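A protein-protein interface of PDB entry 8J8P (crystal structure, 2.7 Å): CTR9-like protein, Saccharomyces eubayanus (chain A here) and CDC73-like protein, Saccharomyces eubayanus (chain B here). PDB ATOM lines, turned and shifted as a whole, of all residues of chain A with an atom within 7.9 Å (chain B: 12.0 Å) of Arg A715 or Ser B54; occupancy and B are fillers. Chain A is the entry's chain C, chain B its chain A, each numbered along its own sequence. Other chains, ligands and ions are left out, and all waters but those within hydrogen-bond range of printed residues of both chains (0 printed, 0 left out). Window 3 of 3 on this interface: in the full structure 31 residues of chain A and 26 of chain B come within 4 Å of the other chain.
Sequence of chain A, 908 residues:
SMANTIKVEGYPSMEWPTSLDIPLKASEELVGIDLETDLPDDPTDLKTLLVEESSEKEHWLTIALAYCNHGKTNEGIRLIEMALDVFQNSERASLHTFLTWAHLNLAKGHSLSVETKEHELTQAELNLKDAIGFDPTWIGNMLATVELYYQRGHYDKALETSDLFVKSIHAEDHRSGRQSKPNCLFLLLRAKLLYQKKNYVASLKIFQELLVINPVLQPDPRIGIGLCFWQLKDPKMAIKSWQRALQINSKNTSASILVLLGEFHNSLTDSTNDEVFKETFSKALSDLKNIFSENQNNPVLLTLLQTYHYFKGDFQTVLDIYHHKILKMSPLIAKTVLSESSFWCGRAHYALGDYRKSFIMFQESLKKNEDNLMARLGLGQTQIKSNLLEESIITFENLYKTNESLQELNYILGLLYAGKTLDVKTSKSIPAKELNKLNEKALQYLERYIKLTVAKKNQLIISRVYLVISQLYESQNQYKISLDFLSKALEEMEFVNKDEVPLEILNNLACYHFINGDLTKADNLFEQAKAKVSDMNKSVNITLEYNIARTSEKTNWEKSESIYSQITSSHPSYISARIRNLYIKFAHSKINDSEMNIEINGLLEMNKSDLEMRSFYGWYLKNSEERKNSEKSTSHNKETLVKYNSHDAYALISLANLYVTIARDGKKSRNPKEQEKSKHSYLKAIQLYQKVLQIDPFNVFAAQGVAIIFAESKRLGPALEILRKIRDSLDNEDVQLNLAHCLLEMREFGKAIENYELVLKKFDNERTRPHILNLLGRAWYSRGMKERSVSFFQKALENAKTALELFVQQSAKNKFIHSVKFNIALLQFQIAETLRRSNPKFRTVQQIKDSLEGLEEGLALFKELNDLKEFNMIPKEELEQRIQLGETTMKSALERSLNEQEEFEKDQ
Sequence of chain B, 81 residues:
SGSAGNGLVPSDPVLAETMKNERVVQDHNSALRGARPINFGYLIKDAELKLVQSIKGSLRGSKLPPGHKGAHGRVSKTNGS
Printed residues of chain B within 4 Å of Leu A683: Leu B51 (3.7 Å). No residue of chain B comes within 4 Å of Phe A710. No residue of chain B comes within 4 Å of Ser A713. No residue of chain B comes within 4 Å of Lys A714. Arg A715 touches two residues of chain B. No residue of chain B comes within 4 Å of Leu A716. No residue of chain B comes within 4 Å of Gly A717. No residue of chain B comes within 4 Å of Pro A718. Of the printed residues of chain A, Ala B47 touches Ile A686. Of the printed residues of chain A, Lys B50 touches Arg A715 (3.3 Å). Of the printed residues of chain A, Gly B57 touches Lys A679 (3.0 Å). The nearest residue of chain B that does not touch Arg A715 is Gln B53 (4.4 Å). The nearest residue of chain A that does not touch Ser B54 is Ser A713 (4.9 Å). The nearest printed residue of chain B that does not touch Lys A679 is Ile B55 (4.3 Å).
CG of Leu B51 touches CD1 of Leu A683, at 3.7 Å. Ile A686 touches Ala B47 (CG2 to CB, 3.7 Å). CD1 of Leu B51 touches CG2 of Ile A686 (3.5 Å). Leu B43 touches Val A706. Arg A715 touches Ser B54.
The side-chain amino group of Lys A679 sits at hydrogen-bond distance from the backbone carbonyl oxygen of Gly B57, at 3.0 Å. The backbone carbonyl oxygen (O) of Lys B50 sits at hydrogen-bond distance from the guanidinium group (NH1) of Arg A715, 3.3 Å away.
O of Phe A710 lies within hydrogen-bond range of N of Arg A715, at 3.2 Å.
Of the 16 printed residues of chain B, 6 touch a printed residue of chain A. Hydrophobic or aromatic side chains of chain B that line the printed part of chain A: Leu B43, Ala B47 and Leu B51. Of the 20 printed residues of chain A, 5 touch a printed residue of chain B. Along chain A the printed residues that touch a printed residue of chain B span positions 679 to 715. Among the printed residues, 7 pairs touch across the chains. Among the printed residues, no Asp or Glu carboxylate lies within 4 Å of a Lys or Arg side-chain nitrogen of the other chain.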
ATOM      1  N   LYS A 667      25.553  -5.469 -13.130  1.00  0.00           N
ATOM      2  CA  LYS A 667      26.280  -4.401 -12.445  1.00  0.00           C
ATOM      3  C   LYS A 667      26.860  -4.827 -11.101  1.00  0.00           C
ATOM      4  O   LYS A 667      27.725  -4.123 -10.569  1.00  0.00           O
ATOM      5  CB  LYS A 667      25.368  -3.189 -12.228  1.00  0.00           C
ATOM      6  CG  LYS A 667      25.509  -2.085 -13.263  1.00  0.00           C
ATOM      7  CD  LYS A 667      24.638  -0.894 -12.898  1.00  0.00           C
ATOM      8  CE  LYS A 667      24.802   0.238 -13.891  1.00  0.00           C
ATOM      9  NZ  LYS A 667      23.622   1.145 -13.887  1.00  0.00           N
ATOM     10  N   LYS A 679      25.734  -2.491 -19.423  1.00  0.00           N
ATOM     11  CA  LYS A 679      25.469  -1.273 -20.195  1.00  0.00           C
ATOM     12  C   LYS A 679      24.811  -1.561 -21.575  1.00  0.00           C
ATOM     13  O   LYS A 679      24.664  -0.626 -22.378  1.00  0.00           O
ATOM     14  CB  LYS A 679      26.759  -0.473 -20.393  1.00  0.00           C
ATOM     15  CG  LYS A 679      27.222   0.282 -19.156  1.00  0.00           C
ATOM     16  CD  LYS A 679      28.625   0.831 -19.338  1.00  0.00           C
ATOM     17  CE  LYS A 679      29.174   1.380 -18.035  1.00  0.00           C
ATOM     18  NZ  LYS A 679      30.610   1.736 -18.174  1.00  0.00           N
ATOM     19  N   LEU A 683      20.349  -0.428 -21.862  1.00  0.00           N
ATOM     20  CA  LEU A 683      19.843   0.389 -22.958  1.00  0.00           C
ATOM     21  C   LEU A 683      18.920  -0.383 -23.895  1.00  0.00           C
ATOM     22  O   LEU A 683      18.222   0.242 -24.693  1.00  0.00           O
ATOM     23  CB  LEU A 683      20.998   1.001 -23.753  1.00  0.00           C
ATOM     24  CG  LEU A 683      20.756   2.456 -24.173  1.00  0.00           C
ATOM     25  CD1 LEU A 683      20.175   3.255 -22.993  1.00  0.00           C
ATOM     26  CD2 LEU A 683      22.001   3.133 -24.758  1.00  0.00           C
ATOM     27  N   ILE A 686      15.490   1.060 -22.731  1.00  0.00           N
ATOM     28  CA  ILE A 686      15.056   2.307 -23.338  1.00  0.00           C
ATOM     29  C   ILE A 686      15.044   2.238 -24.868  1.00  0.00           C
ATOM     30  O   ILE A 686      14.461   3.114 -25.514  1.00  0.00           O
ATOM     31  CB  ILE A 686      15.932   3.450 -22.782  1.00  0.00           C
ATOM     32  CG1 ILE A 686      16.133   3.266 -21.269  1.00  0.00           C
ATOM     33  CG2 ILE A 686      15.285   4.801 -23.038  1.00  0.00           C
ATOM     34  CD1 ILE A 686      17.466   3.766 -20.744  1.00  0.00           C
ATOM     35  N   VAL A 706      10.430   2.911 -16.985  1.00  0.00           N
ATOM     36  CA  VAL A 706      11.238   4.088 -16.674  1.00  0.00           C
ATOM     37  C   VAL A 706      11.398   4.217 -15.167  1.00  0.00           C
ATOM     38  O   VAL A 706      12.510   4.422 -14.659  1.00  0.00           O
ATOM     39  CB  VAL A 706      10.596   5.359 -17.263  1.00  0.00           C
ATOM     40  CG1 VAL A 706      10.963   6.588 -16.436  1.00  0.00           C
ATOM     41  CG2 VAL A 706      11.009   5.543 -18.714  1.00  0.00           C
ATOM     42  N   ALA A 707      10.284   4.062 -14.448  1.00  0.00           N
ATOM     43  CA  ALA A 707      10.291   4.198 -12.997  1.00  0.00           C
ATOM     44  C   ALA A 707      11.350   3.305 -12.366  1.00  0.00           C
ATOM     45  O   ALA A 707      12.255   3.786 -11.673  1.00  0.00           O
ATOM     46  CB  ALA A 707       8.912   3.864 -12.441  1.00  0.00           C
ATOM     47  N   ILE A 709      13.856   2.071 -13.457  1.00  0.00           N
ATOM     48  CA  ILE A 709      15.233   2.401 -13.805  1.00  0.00           C
ATOM     49  C   ILE A 709      15.809   3.377 -12.785  1.00  0.00           C
ATOM     50  O   ILE A 709      16.943   3.209 -12.318  1.00  0.00           O
ATOM     51  CB  ILE A 709      15.327   2.957 -15.240  1.00  0.00           C
ATOM     52  CG1 ILE A 709      15.532   1.831 -16.259  1.00  0.00           C
ATOM     53  CG2 ILE A 709      16.494   3.919 -15.371  1.00  0.00           C
ATOM     54  CD1 ILE A 709      14.325   0.966 -16.508  1.00  0.00           C
ATOM     55  N   PHE A 710      15.025   4.380 -12.386  1.00  0.00           N
ATOM     56  CA  PHE A 710      15.591   5.477 -11.607  1.00  0.00           C
ATOM     57  C   PHE A 710      15.834   5.073 -10.154  1.00  0.00           C
ATOM     58  O   PHE A 710      16.853   5.452  -9.568  1.00  0.00           O
ATOM     59  CB  PHE A 710      14.686   6.710 -11.680  1.00  0.00           C
ATOM     60  CG  PHE A 710      14.493   7.273 -13.080  1.00  0.00           C
ATOM     61  CD1 PHE A 710      15.016   6.639 -14.195  1.00  0.00           C
ATOM     62  CD2 PHE A 710      13.787   8.452 -13.269  1.00  0.00           C
ATOM     63  CE1 PHE A 710      14.830   7.157 -15.465  1.00  0.00           C
ATOM     64  CE2 PHE A 710      13.600   8.978 -14.537  1.00  0.00           C
ATOM     65  CZ  PHE A 710      14.123   8.330 -15.637  1.00  0.00           C
ATOM     66  N   ALA A 711      14.922   4.298  -9.556  1.00  0.00           N
ATOM     67  CA  ALA A 711      15.216   3.695  -8.258  1.00  0.00           C
ATOM     68  C   ALA A 711      16.425   2.772  -8.335  1.00  0.00           C
ATOM     69  O   ALA A 711      17.035   2.471  -7.302  1.00  0.00           O
ATOM     70  CB  ALA A 711      13.998   2.927  -7.730  1.00  0.00           C
ATOM     71  N   GLU A 712      16.788   2.336  -9.542  1.00  0.00           N
ATOM     72  CA  GLU A 712      17.930   1.469  -9.794  1.00  0.00           C
ATOM     73  C   GLU A 712      19.145   2.223 -10.318  1.00  0.00           C
ATOM     74  O   GLU A 712      20.279   1.803 -10.061  1.00  0.00           O
ATOM     75  CB  GLU A 712      17.534   0.378 -10.799  1.00  0.00           C
ATOM     76  CG  GLU A 712      18.567  -0.710 -11.045  1.00  0.00           C
ATOM     77  CD  GLU A 712      17.960  -1.945 -11.693  1.00  0.00           C
ATOM     78  OE1 GLU A 712      18.568  -2.485 -12.640  1.00  0.00           O
ATOM     79  OE2 GLU A 712      16.873  -2.377 -11.252  1.00  0.00           O
ATOM     80  N   SER A 713      18.937   3.329 -11.037  1.00  0.00           N
ATOM     81  CA  SER A 713      20.022   4.110 -11.621  1.00  0.00           C
ATOM     82  C   SER A 713      20.243   5.443 -10.913  1.00  0.00           C
ATOM     83  O   SER A 713      21.013   6.278 -11.407  1.00  0.00           O
ATOM     84  CB  SER A 713      19.766   4.341 -13.112  1.00  0.00           C
ATOM     85  OG  SER A 713      20.663   5.299 -13.644  1.00  0.00           O
ATOM     86  N   LYS A 714      19.585   5.658  -9.773  1.00  0.00           N
ATOM     87  CA  LYS A 714      19.846   6.795  -8.893  1.00  0.00           C
ATOM     88  C   LYS A 714      19.575   8.128  -9.603  1.00  0.00           C
ATOM     89  O   LYS A 714      20.455   8.973  -9.781  1.00  0.00           O
ATOM     90  CB  LYS A 714      21.272   6.701  -8.347  1.00  0.00           C
ATOM     91  CG  LYS A 714      21.474   5.461  -7.484  1.00  0.00           C
ATOM     92  CD  LYS A 714      22.944   5.127  -7.313  1.00  0.00           C
ATOM     93  CE  LYS A 714      23.403   4.155  -8.371  1.00  0.00           C
ATOM     94  NZ  LYS A 714      24.790   4.418  -8.789  1.00  0.00           N
ATOM     95  N   ARG A 715      18.327   8.271 -10.053  1.00  0.00           N
ATOM     96  CA  ARG A 715      17.806   9.535 -10.563  1.00  0.00           C
ATOM     97  C   ARG A 715      16.365   9.697 -10.093  1.00  0.00           C
ATOM     98  O   ARG A 715      15.479  10.090 -10.858  1.00  0.00           O
ATOM     99  CB  ARG A 715      17.900   9.610 -12.091  1.00  0.00           C
ATOM    100  CG  ARG A 715      19.320   9.512 -12.642  1.00  0.00           C
ATOM    101  CD  ARG A 715      19.339   9.667 -14.143  1.00  0.00           C
ATOM    102  NE  ARG A 715      19.397  11.071 -14.531  1.00  0.00           N
ATOM    103  CZ  ARG A 715      19.854  11.499 -15.701  1.00  0.00           C
ATOM    104  NH1 ARG A 715      20.293  10.625 -16.598  1.00  0.00           N
ATOM    105  NH2 ARG A 715      19.868  12.797 -15.976  1.00  0.00           N
ATOM    106  N   LEU A 716      16.135   9.410  -8.808  1.00  0.00           N
ATOM    107  CA  LEU A 716      14.797   9.112  -8.313  1.00  0.00           C
ATOM    108  C   LEU A 716      13.903  10.344  -8.276  1.00  0.00           C
ATOM    109  O   LEU A 716      12.682  10.217  -8.408  1.00  0.00           O
ATOM    110  CB  LEU A 716      14.884   8.489  -6.919  1.00  0.00           C
ATOM    111  CG  LEU A 716      15.836   7.307  -6.693  1.00  0.00           C
ATOM    112  CD1 LEU A 716      17.243   7.764  -6.321  1.00  0.00           C
ATOM    113  CD2 LEU A 716      15.280   6.355  -5.644  1.00  0.00           C
ATOM    114  N   GLY A 717      14.476  11.531  -8.084  1.00  0.00           N
ATOM    115  CA  GLY A 717      13.719  12.765  -8.038  1.00  0.00           C
ATOM    116  C   GLY A 717      12.702  12.892  -9.156  1.00  0.00           C
ATOM    117  O   GLY A 717      11.496  13.038  -8.927  1.00  0.00           O
ATOM    118  N   PRO A 718      13.185  12.865 -10.398  1.00  0.00           N
ATOM    119  CA  PRO A 718      12.265  12.794 -11.544  1.00  0.00           C
ATOM    120  C   PRO A 718      11.300  11.611 -11.497  1.00  0.00           C
ATOM    121  O   PRO A 718      10.201  11.717 -12.053  1.00  0.00           O
ATOM    122  CB  PRO A 718      13.218  12.692 -12.743  1.00  0.00           C
ATOM    123  CG  PRO A 718      14.465  13.391 -12.294  1.00  0.00           C
ATOM    124  CD  PRO A 718      14.575  13.139 -10.811  1.00  0.00           C
ATOM    125  N   ALA A 719      11.661  10.507 -10.832  1.00  0.00           N
ATOM    126  CA  ALA A 719      10.945   9.236 -10.948  1.00  0.00           C
ATOM    127  C   ALA A 719       9.679   9.156 -10.106  1.00  0.00           C
ATOM    128  O   ALA A 719       8.639   8.706 -10.606  1.00  0.00           O
ATOM    129  CB  ALA A 719      11.856   8.069 -10.559  1.00  0.00           C
ATOM    130  N   LEU A 720       9.751   9.546  -8.828  1.00  0.00           N
ATOM    131  CA  LEU A 720       8.578   9.434  -7.971  1.00  0.00           C
ATOM    132  C   LEU A 720       7.493  10.413  -8.394  1.00  0.00           C
ATOM    133  O   LEU A 720       6.341  10.263  -8.006  1.00  0.00           O
ATOM    134  CB  LEU A 720       8.967   9.635  -6.507  1.00  0.00           C
ATOM    135  CG  LEU A 720       8.877  11.009  -5.839  1.00  0.00           C
ATOM    136  CD1 LEU A 720       9.046  10.863  -4.327  1.00  0.00           C
ATOM    137  CD2 LEU A 720       9.906  11.987  -6.381  1.00  0.00           C
ATOM    138  N   ILE A 722       6.689  10.441 -11.728  1.00  0.00           N
ATOM    139  CA  ILE A 722       5.979   9.483 -12.571  1.00  0.00           C
ATOM    140  C   ILE A 722       5.206   8.488 -11.716  1.00  0.00           C
ATOM    141  O   ILE A 722       4.083   8.111 -12.068  1.00  0.00           O
ATOM    142  CB  ILE A 722       6.905   8.742 -13.572  1.00  0.00           C
ATOM    143  CG1 ILE A 722       7.814   9.695 -14.395  1.00  0.00           C
ATOM    144  CG2 ILE A 722       6.063   7.814 -14.488  1.00  0.00           C
ATOM    145  CD1 ILE A 722       9.349   9.598 -14.142  1.00  0.00           C
ATOM    146  N   CYS A 742      11.521   3.704  -4.228  1.00  0.00           N
ATOM    147  CA  CYS A 742      12.127   4.952  -4.674  1.00  0.00           C
ATOM    148  C   CYS A 742      12.058   6.009  -3.583  1.00  0.00           C
ATOM    149  O   CYS A 742      12.965   6.837  -3.443  1.00  0.00           O
ATOM    150  CB  CYS A 742      11.430   5.446  -5.947  1.00  0.00           C
ATOM    151  SG  CYS A 742      11.657   7.202  -6.334  1.00  0.00           S
ATOM    152  N   TYR B  42       5.384  12.522 -22.829  1.00  0.00           N
ATOM    153  CA  TYR B  42       6.515  13.346 -22.428  1.00  0.00           C
ATOM    154  C   TYR B  42       7.751  12.497 -22.158  1.00  0.00           C
ATOM    155  O   TYR B  42       8.888  12.971 -22.326  1.00  0.00           O
ATOM    156  CB  TYR B  42       6.110  14.195 -21.216  1.00  0.00           C
ATOM    157  CG  TYR B  42       5.647  13.430 -19.979  1.00  0.00           C
ATOM    158  CD1 TYR B  42       6.562  12.707 -19.198  1.00  0.00           C
ATOM    159  CD2 TYR B  42       4.299  13.419 -19.596  1.00  0.00           C
ATOM    160  CE1 TYR B  42       6.149  12.014 -18.059  1.00  0.00           C
ATOM    161  CE2 TYR B  42       3.881  12.740 -18.479  1.00  0.00           C
ATOM    162  CZ  TYR B  42       4.778  12.047 -17.710  1.00  0.00           C
ATOM    163  OH  TYR B  42       4.319  11.377 -16.604  1.00  0.00           O
ATOM    164  N   LEU B  43       7.544  11.228 -21.800  1.00  0.00           N
ATOM    165  CA  LEU B  43       8.647  10.349 -21.438  1.00  0.00           C
ATOM    166  C   LEU B  43       9.475   9.846 -22.620  1.00  0.00           C
ATOM    167  O   LEU B  43      10.610   9.434 -22.394  1.00  0.00           O
ATOM    168  CB  LEU B  43       8.130   9.174 -20.614  1.00  0.00           C
ATOM    169  CG  LEU B  43       8.043   9.433 -19.093  1.00  0.00           C
ATOM    170  CD1 LEU B  43       7.902   8.120 -18.339  1.00  0.00           C
ATOM    171  CD2 LEU B  43       9.305  10.109 -18.659  1.00  0.00           C
ATOM    172  N   ILE B  44       9.004   9.938 -23.868  1.00  0.00           N
ATOM    173  CA  ILE B  44       9.883   9.583 -24.994  1.00  0.00           C
ATOM    174  C   ILE B  44      11.080  10.526 -25.061  1.00  0.00           C
ATOM    175  O   ILE B  44      12.245  10.096 -25.106  1.00  0.00           O
ATOM    176  CB  ILE B  44       9.110   9.569 -26.329  1.00  0.00           C
ATOM    177  CG1 ILE B  44      10.058   9.267 -27.501  1.00  0.00           C
ATOM    178  CG2 ILE B  44       8.304  10.840 -26.545  1.00  0.00           C
ATOM    179  CD1 ILE B  44      10.268   7.794 -27.714  1.00  0.00           C
ATOM    180  N   LYS B  45      10.811  11.832 -25.058  1.00  0.00           N
ATOM    181  CA  LYS B  45      11.896  12.798 -25.094  1.00  0.00           C
ATOM    182  C   LYS B  45      12.626  12.858 -23.761  1.00  0.00           C
ATOM    183  O   LYS B  45      13.854  13.006 -23.747  1.00  0.00           O
ATOM    184  CB  LYS B  45      11.361  14.171 -25.502  1.00  0.00           C
ATOM    185  CG  LYS B  45      10.417  14.116 -26.695  1.00  0.00           C
ATOM    186  CD  LYS B  45       8.983  14.371 -26.272  1.00  0.00           C
ATOM    187  CE  LYS B  45       8.050  14.400 -27.468  1.00  0.00           C
ATOM    188  NZ  LYS B  45       6.677  14.802 -27.060  1.00  0.00           N
ATOM    189  N   ASP B  46      11.911  12.723 -22.635  1.00  0.00           N
ATOM    190  CA  ASP B  46      12.602  12.643 -21.348  1.00  0.00           C
ATOM    191  C   ASP B  46      13.637  11.520 -21.349  1.00  0.00           C
ATOM    192  O   ASP B  46      14.788  11.714 -20.928  1.00  0.00           O
ATOM    193  CB  ASP B  46      11.592  12.450 -20.217  1.00  0.00           C
ATOM    194  CG  ASP B  46      10.993  13.762 -19.739  1.00  0.00           C
ATOM    195  OD1 ASP B  46      10.693  14.626 -20.591  1.00  0.00           O
ATOM    196  OD2 ASP B  46      10.825  13.932 -18.511  1.00  0.00           O
ATOM    197  N   ALA B  47      13.247  10.338 -21.837  1.00  0.00           N
ATOM    198  CA  ALA B  47      14.152   9.216 -22.015  1.00  0.00           C
ATOM    199  C   ALA B  47      15.320   9.612 -22.900  1.00  0.00           C
ATOM    200  O   ALA B  47      16.432   9.755 -22.403  1.00  0.00           O
ATOM    201  CB  ALA B  47      13.410   8.012 -22.602  1.00  0.00           C
ATOM    202  N   GLU B  48      15.077   9.861 -24.191  1.00  0.00           N
ATOM    203  CA  GLU B  48      16.202  10.074 -25.107  1.00  0.00           C
ATOM    204  C   GLU B  48      17.081  11.265 -24.706  1.00  0.00           C
ATOM    205  O   GLU B  48      18.202  11.395 -25.205  1.00  0.00           O
ATOM    206  CB  GLU B  48      15.702  10.217 -26.551  1.00  0.00           C
ATOM    207  CG  GLU B  48      16.777  10.541 -27.596  1.00  0.00           C
ATOM    208  CD  GLU B  48      17.319   9.292 -28.269  1.00  0.00           C
ATOM    209  OE1 GLU B  48      17.118   8.197 -27.701  1.00  0.00           O
ATOM    210  OE2 GLU B  48      17.968   9.404 -29.335  1.00  0.00           O
ATOM    211  N   LEU B  49      16.640  12.109 -23.771  1.00  0.00           N
ATOM    212  CA  LEU B  49      17.575  13.043 -23.143  1.00  0.00           C
ATOM    213  C   LEU B  49      18.402  12.352 -22.059  1.00  0.00           C
ATOM    214  O   LEU B  49      19.635  12.352 -22.124  1.00  0.00           O
ATOM    215  CB  LEU B  49      16.841  14.261 -22.559  1.00  0.00           C
ATOM    216  CG  LEU B  49      15.992  15.175 -23.443  1.00  0.00           C
ATOM    217  CD1 LEU B  49      15.156  16.133 -22.593  1.00  0.00           C
ATOM    218  CD2 LEU B  49      16.848  15.940 -24.444  1.00  0.00           C
ATOM    219  N   LYS B  50      17.740  11.734 -21.067  1.00  0.00           N
ATOM    220  CA  LYS B  50      18.461  11.211 -19.902  1.00  0.00           C
ATOM    221  C   LYS B  50      19.308   9.987 -20.258  1.00  0.00           C
ATOM    222  O   LYS B  50      20.446   9.861 -19.789  1.00  0.00           O
ATOM    223  CB  LYS B  50      17.470  10.885 -18.783  1.00  0.00           C
ATOM    224  CG  LYS B  50      17.129  12.055 -17.833  1.00  0.00           C
ATOM    225  CD  LYS B  50      16.892  13.384 -18.557  1.00  0.00           C
ATOM    226  CE  LYS B  50      16.346  14.451 -17.611  1.00  0.00           C
ATOM    227  NZ  LYS B  50      14.891  14.275 -17.327  1.00  0.00           N
ATOM    228  N   LEU B  51      18.745   9.056 -21.036  1.00  0.00           N
ATOM    229  CA  LEU B  51      19.446   8.012 -21.781  1.00  0.00           C
ATOM    230  C   LEU B  51      20.828   8.457 -22.235  1.00  0.00           C
ATOM    231  O   LEU B  51      21.854   7.957 -21.756  1.00  0.00           O
ATOM    232  CB  LEU B  51      18.616   7.630 -23.022  1.00  0.00           C
ATOM    233  CG  LEU B  51      18.975   6.552 -24.069  1.00  0.00           C
ATOM    234  CD1 LEU B  51      17.779   6.264 -24.975  1.00  0.00           C
ATOM    235  CD2 LEU B  51      20.197   6.856 -24.943  1.00  0.00           C
ATOM    236  N   VAL B  52      20.837   9.392 -23.190  1.00  0.00           N
ATOM    237  CA  VAL B  52      22.057   9.779 -23.885  1.00  0.00           C
ATOM    238  C   VAL B  52      22.970  10.566 -22.961  1.00  0.00           C
ATOM    239  O   VAL B  52      24.200  10.512 -23.097  1.00  0.00           O
ATOM    240  CB  VAL B  52      21.698  10.569 -25.162  1.00  0.00           C
ATOM    241  CG1 VAL B  52      21.369  12.034 -24.848  1.00  0.00           C
ATOM    242  CG2 VAL B  52      22.789  10.456 -26.211  1.00  0.00           C
ATOM    243  N   GLN B  53      22.399  11.293 -21.996  1.00  0.00           N
ATOM    244  CA  GLN B  53      23.233  12.031 -21.058  1.00  0.00           C
ATOM    245  C   GLN B  53      23.910  11.112 -20.050  1.00  0.00           C
ATOM    246  O   GLN B  53      24.943  11.487 -19.488  1.00  0.00           O
ATOM    247  CB  GLN B  53      22.398  13.092 -20.339  1.00  0.00           C
ATOM    248  CG  GLN B  53      21.949  14.238 -21.238  1.00  0.00           C
ATOM    249  CD  GLN B  53      21.517  15.462 -20.457  1.00  0.00           C
ATOM    250  OE1 GLN B  53      20.808  15.354 -19.453  1.00  0.00           O
ATOM    251  NE2 GLN B  53      21.928  16.638 -20.922  1.00  0.00           N
ATOM    252  N   SER B  54      23.365   9.917 -19.822  1.00  0.00           N
ATOM    253  CA  SER B  54      23.945   8.976 -18.856  1.00  0.00           C
ATOM    254  C   SER B  54      24.957   8.038 -19.517  1.00  0.00           C
ATOM    255  O   SER B  54      26.160   8.170 -19.305  1.00  0.00           O
ATOM    256  CB  SER B  54      22.835   8.193 -18.152  1.00  0.00           C
ATOM    257  OG  SER B  54      23.359   7.287 -17.197  1.00  0.00           O
ATOM    258  N   ILE B  55      24.473   7.095 -20.326  1.00  0.00           N
ATOM    259  CA  ILE B  55      25.279   5.947 -20.740  1.00  0.00           C
ATOM    260  C   ILE B  55      26.152   6.326 -21.934  1.00  0.00           C
ATOM    261  O   ILE B  55      25.698   6.267 -23.075  1.00  0.00           O
ATOM    262  CB  ILE B  55      24.387   4.745 -21.076  1.00  0.00           C
ATOM    263  CG1 ILE B  55      23.385   4.499 -19.940  1.00  0.00           C
ATOM    264  CG2 ILE B  55      25.229   3.495 -21.336  1.00  0.00           C
ATOM    265  CD1 ILE B  55      24.025   4.182 -18.599  1.00  0.00           C
ATOM    266  N   LYS B  56      27.413   6.681 -21.684  1.00  0.00           N
ATOM    267  CA  LYS B  56      28.387   6.962 -22.743  1.00  0.00           C
ATOM    268  C   LYS B  56      29.547   5.968 -22.656  1.00  0.00           C
ATOM    269  O   LYS B  56      30.717   6.324 -22.746  1.00  0.00           O
ATOM    270  CB  LYS B  56      28.885   8.411 -22.665  1.00  0.00           C
ATOM    271  CG  LYS B  56      27.886   9.525 -23.108  1.00  0.00           C
ATOM    272  CD  LYS B  56      27.490   9.474 -24.589  1.00  0.00           C
ATOM    273  CE  LYS B  56      26.197   8.678 -24.802  1.00  0.00           C
ATOM    274  NZ  LYS B  56      25.529   9.003 -26.107  1.00  0.00           N
ATOM    275  N   GLY B  57      29.242   4.689 -22.517  1.00  0.00           N
ATOM    276  CA  GLY B  57      30.271   3.687 -22.297  1.00  0.00           C
ATOM    277  C   GLY B  57      30.477   3.463 -20.814  1.00  0.00           C
ATOM    278  O   GLY B  57      29.651   3.892 -19.999  1.00  0.00           O
